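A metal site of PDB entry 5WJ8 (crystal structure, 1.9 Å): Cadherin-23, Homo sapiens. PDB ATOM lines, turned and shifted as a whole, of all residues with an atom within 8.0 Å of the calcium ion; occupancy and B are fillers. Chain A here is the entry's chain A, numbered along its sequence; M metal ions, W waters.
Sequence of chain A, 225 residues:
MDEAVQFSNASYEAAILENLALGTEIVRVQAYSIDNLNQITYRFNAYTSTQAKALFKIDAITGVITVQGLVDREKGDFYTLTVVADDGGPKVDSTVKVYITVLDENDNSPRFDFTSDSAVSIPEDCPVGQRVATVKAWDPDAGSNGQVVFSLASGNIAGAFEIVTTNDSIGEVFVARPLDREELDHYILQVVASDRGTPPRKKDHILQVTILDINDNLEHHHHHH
Water W2 lies within hydrogen-bond range of the side-chain carboxylate (OD1) of Asp 86, the backbone NH (N) of Gly 88 and the backbone NH (N) of Gly 89.
The side-chain amide nitrogen of Asn 38 is in hydrogen-bond range of the backbone carbonyl oxygen of Asp 87.
The calcium ion is bound by water W1 (2.3 Å), O of Lys 91 (2.3 Å), O of Gly 89 (2.3 Å), OD1 of Asp 87 (2.3 Å), water W2 (2.4 Å), OD2 of Asp 93 (2.5 Å) and OD1 of Asp 93 (2.6 Å). The calcium ion has seven donor atoms within binding distance.
Within 4 Å of the calcium ion: Asp 87, Gly 89, Lys 91 and Asp 93. The nearest printed residue that does not touch the calcium ion is Pro 90 (4.2 Å).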
ATOM      1  N   ASN A  36      12.685  -2.632  26.298  1.00  0.00           N
ATOM      2  CA  ASN A  36      11.363  -3.031  25.815  1.00  0.00           C
ATOM      3  C   ASN A  36      11.547  -4.345  25.081  1.00  0.00           C
ATOM      4  O   ASN A  36      12.106  -4.340  23.983  1.00  0.00           O
ATOM      5  CB  ASN A  36      10.789  -1.958  24.852  1.00  0.00           C
ATOM      6  CG  ASN A  36       9.620  -2.470  24.007  1.00  0.00           C
ATOM      7  OD1 ASN A  36       8.511  -2.698  24.522  1.00  0.00           O
ATOM      8  ND2 ASN A  36       9.852  -2.664  22.707  1.00  0.00           N
ATOM      9  N   ASN A  38       8.974  -6.399  24.089  1.00  0.00           N
ATOM     10  CA  ASN A  38       7.826  -6.770  23.249  1.00  0.00           C
ATOM     11  C   ASN A  38       8.152  -6.554  21.784  1.00  0.00           C
ATOM     12  O   ASN A  38       8.782  -5.565  21.438  1.00  0.00           O
ATOM     13  CB  ASN A  38       6.555  -5.968  23.624  1.00  0.00           C
ATOM     14  CG  ASN A  38       5.918  -6.444  24.922  1.00  0.00           C
ATOM     15  OD1 ASN A  38       6.441  -7.341  25.589  1.00  0.00           O
ATOM     16  ND2 ASN A  38       4.771  -5.843  25.305  1.00  0.00           N
ATOM     17  N   ARG A  43       1.117   0.180  13.132  1.00  0.00           N
ATOM     18  CA  ARG A  43      -0.259   0.400  12.654  1.00  0.00           C
ATOM     19  C   ARG A  43      -0.512   1.882  12.460  1.00  0.00           C
ATOM     20  O   ARG A  43       0.150   2.697  13.093  1.00  0.00           O
ATOM     21  CB  ARG A  43      -1.301  -0.194  13.640  1.00  0.00           C
ATOM     22  CG  ARG A  43      -1.276   0.384  15.032  1.00  0.00           C
ATOM     23  CD  ARG A  43      -2.298  -0.294  15.963  1.00  0.00           C
ATOM     24  NE  ARG A  43      -2.201   0.344  17.265  1.00  0.00           N
ATOM     25  CZ  ARG A  43      -2.743   1.521  17.597  1.00  0.00           C
ATOM     26  NH1 ARG A  43      -2.561   2.011  18.823  1.00  0.00           N
ATOM     27  NH2 ARG A  43      -3.473   2.217  16.718  1.00  0.00           N
ATOM     28  N   VAL A  84       1.844   4.219  14.598  1.00  0.00           N
ATOM     29  CA  VAL A  84       2.110   3.947  16.001  1.00  0.00           C
ATOM     30  C   VAL A  84       3.025   2.739  16.083  1.00  0.00           C
ATOM     31  O   VAL A  84       2.763   1.726  15.438  1.00  0.00           O
ATOM     32  CB  VAL A  84       0.802   3.592  16.762  1.00  0.00           C
ATOM     33  CG1 VAL A  84       1.077   3.425  18.250  1.00  0.00           C
ATOM     34  CG2 VAL A  84      -0.241   4.666  16.546  1.00  0.00           C
ATOM     35  N   ALA A  85       4.076   2.851  16.890  1.00  0.00           N
ATOM     36  CA  ALA A  85       4.887   1.691  17.264  1.00  0.00           C
ATOM     37  C   ALA A  85       4.237   1.129  18.535  1.00  0.00           C
ATOM     38  O   ALA A  85       4.577   1.521  19.645  1.00  0.00           O
ATOM     39  CB  ALA A  85       6.340   2.081  17.510  1.00  0.00           C
ATOM     40  N   ASP A  86       3.306   0.197  18.348  1.00  0.00           N
ATOM     41  CA  ASP A  86       2.426  -0.262  19.439  1.00  0.00           C
ATOM     42  C   ASP A  86       3.070  -1.463  20.122  1.00  0.00           C
ATOM     43  O   ASP A  86       3.161  -2.548  19.527  1.00  0.00           O
ATOM     44  CB  ASP A  86       1.058  -0.628  18.859  1.00  0.00           C
ATOM     45  CG  ASP A  86      -0.006  -0.853  19.912  1.00  0.00           C
ATOM     46  OD1 ASP A  86       0.356  -1.237  21.043  1.00  0.00           O
ATOM     47  OD2 ASP A  86      -1.206  -0.673  19.590  1.00  0.00           O
ATOM     48  N   ASP A  87       3.459  -1.291  21.381  1.00  0.00           N
ATOM     49  CA  ASP A  87       4.094  -2.399  22.119  1.00  0.00           C
ATOM     50  C   ASP A  87       3.095  -3.440  22.687  1.00  0.00           C
ATOM     51  O   ASP A  87       3.474  -4.521  23.170  1.00  0.00           O
ATOM     52  CB  ASP A  87       5.090  -1.844  23.156  1.00  0.00           C
ATOM     53  CG  ASP A  87       4.424  -1.289  24.386  1.00  0.00           C
ATOM     54  OD1 ASP A  87       3.173  -1.086  24.400  1.00  0.00           O
ATOM     55  OD2 ASP A  87       5.167  -1.030  25.360  1.00  0.00           O
ATOM     56  N   GLY A  88       1.798  -3.138  22.587  1.00  0.00           N
ATOM     57  CA  GLY A  88       0.778  -4.062  23.091  1.00  0.00           C
ATOM     58  C   GLY A  88       0.661  -4.190  24.617  1.00  0.00           C
ATOM     59  O   GLY A  88      -0.003  -5.104  25.125  1.00  0.00           O
ATOM     60  N   GLY A  89       1.268  -3.249  25.324  1.00  0.00           N
ATOM     61  CA  GLY A  89       1.293  -3.245  26.768  1.00  0.00           C
ATOM     62  C   GLY A  89       1.014  -1.849  27.292  1.00  0.00           C
ATOM     63  O   GLY A  89       0.796  -0.926  26.519  1.00  0.00           O
ATOM     64  N   PRO A  90       1.016  -1.686  28.618  1.00  0.00           N
ATOM     65  CA  PRO A  90       0.549  -0.424  29.204  1.00  0.00           C
ATOM     66  C   PRO A  90       1.398   0.819  28.953  1.00  0.00           C
ATOM     67  O   PRO A  90       0.887   1.923  29.113  1.00  0.00           O
ATOM     68  CB  PRO A  90       0.498  -0.729  30.704  1.00  0.00           C
ATOM     69  CG  PRO A  90       0.395  -2.218  30.778  1.00  0.00           C
ATOM     70  CD  PRO A  90       1.272  -2.697  29.658  1.00  0.00           C
ATOM     71  N   LYS A  91       2.664   0.666  28.566  1.00  0.00           N
ATOM     72  CA  LYS A  91       3.487   1.838  28.274  1.00  0.00           C
ATOM     73  C   LYS A  91       2.899   2.615  27.100  1.00  0.00           C
ATOM     74  O   LYS A  91       2.353   2.020  26.158  1.00  0.00           O
ATOM     75  CB  LYS A  91       4.943   1.488  27.941  1.00  0.00           C
ATOM     76  CG  LYS A  91       5.822   1.245  29.147  1.00  0.00           C
ATOM     77  CD  LYS A  91       7.271   0.964  28.736  1.00  0.00           C
ATOM     78  CE  LYS A  91       8.027   0.290  29.857  1.00  0.00           C
ATOM     79  NZ  LYS A  91       7.624  -1.135  29.992  1.00  0.00           N
ATOM     80  N   VAL A  92       3.015   3.938  27.187  1.00  0.00           N
ATOM     81  CA  VAL A  92       2.550   4.822  26.132  1.00  0.00           C
ATOM     82  C   VAL A  92       3.437   4.582  24.883  1.00  0.00           C
ATOM     83  O   VAL A  92       4.664   4.483  24.983  1.00  0.00           O
ATOM     84  CB  VAL A  92       2.564   6.304  26.566  1.00  0.00           C
ATOM     85  CG1 VAL A  92       2.132   7.215  25.403  1.00  0.00           C
ATOM     86  CG2 VAL A  92       1.661   6.503  27.768  1.00  0.00           C
ATOM     87  N   ASP A  93       2.783   4.480  23.741  1.00  0.00           N
ATOM     88  CA  ASP A  93       3.433   4.104  22.491  1.00  0.00           C
ATOM     89  C   ASP A  93       3.797   5.335  21.688  1.00  0.00           C
ATOM     90  O   ASP A  93       3.025   6.293  21.651  1.00  0.00           O
ATOM     91  CB  ASP A  93       2.510   3.198  21.684  1.00  0.00           C
ATOM     92  CG  ASP A  93       2.118   1.976  22.455  1.00  0.00           C
ATOM     93  OD1 ASP A  93       3.013   1.200  22.860  1.00  0.00           O
ATOM     94  OD2 ASP A  93       0.916   1.791  22.697  1.00  0.00           O
ATOM     95  N   SER A  94       4.948   5.296  21.050  1.00  0.00           N
ATOM     96  CA  SER A  94       5.415   6.419  20.269  1.00  0.00           C
ATOM     97  C   SER A  94       4.764   6.402  18.892  1.00  0.00           C
ATOM     98  O   SER A  94       4.370   5.348  18.378  1.00  0.00           O
ATOM     99  CB  SER A  94       6.935   6.368  20.103  1.00  0.00           C
ATOM    100  OG  SER A  94       7.570   6.285  21.367  1.00  0.00           O
HETATM  101 CA    CA M   1       1.437   0.436  24.774  1.00  0.00          CA
HETATM  102  O   HOH W   1      -0.453   1.598  25.350  1.00  0.00           O
HETATM  103  O   HOH W   2      -0.278  -0.857  23.632  1.00  0.00           O
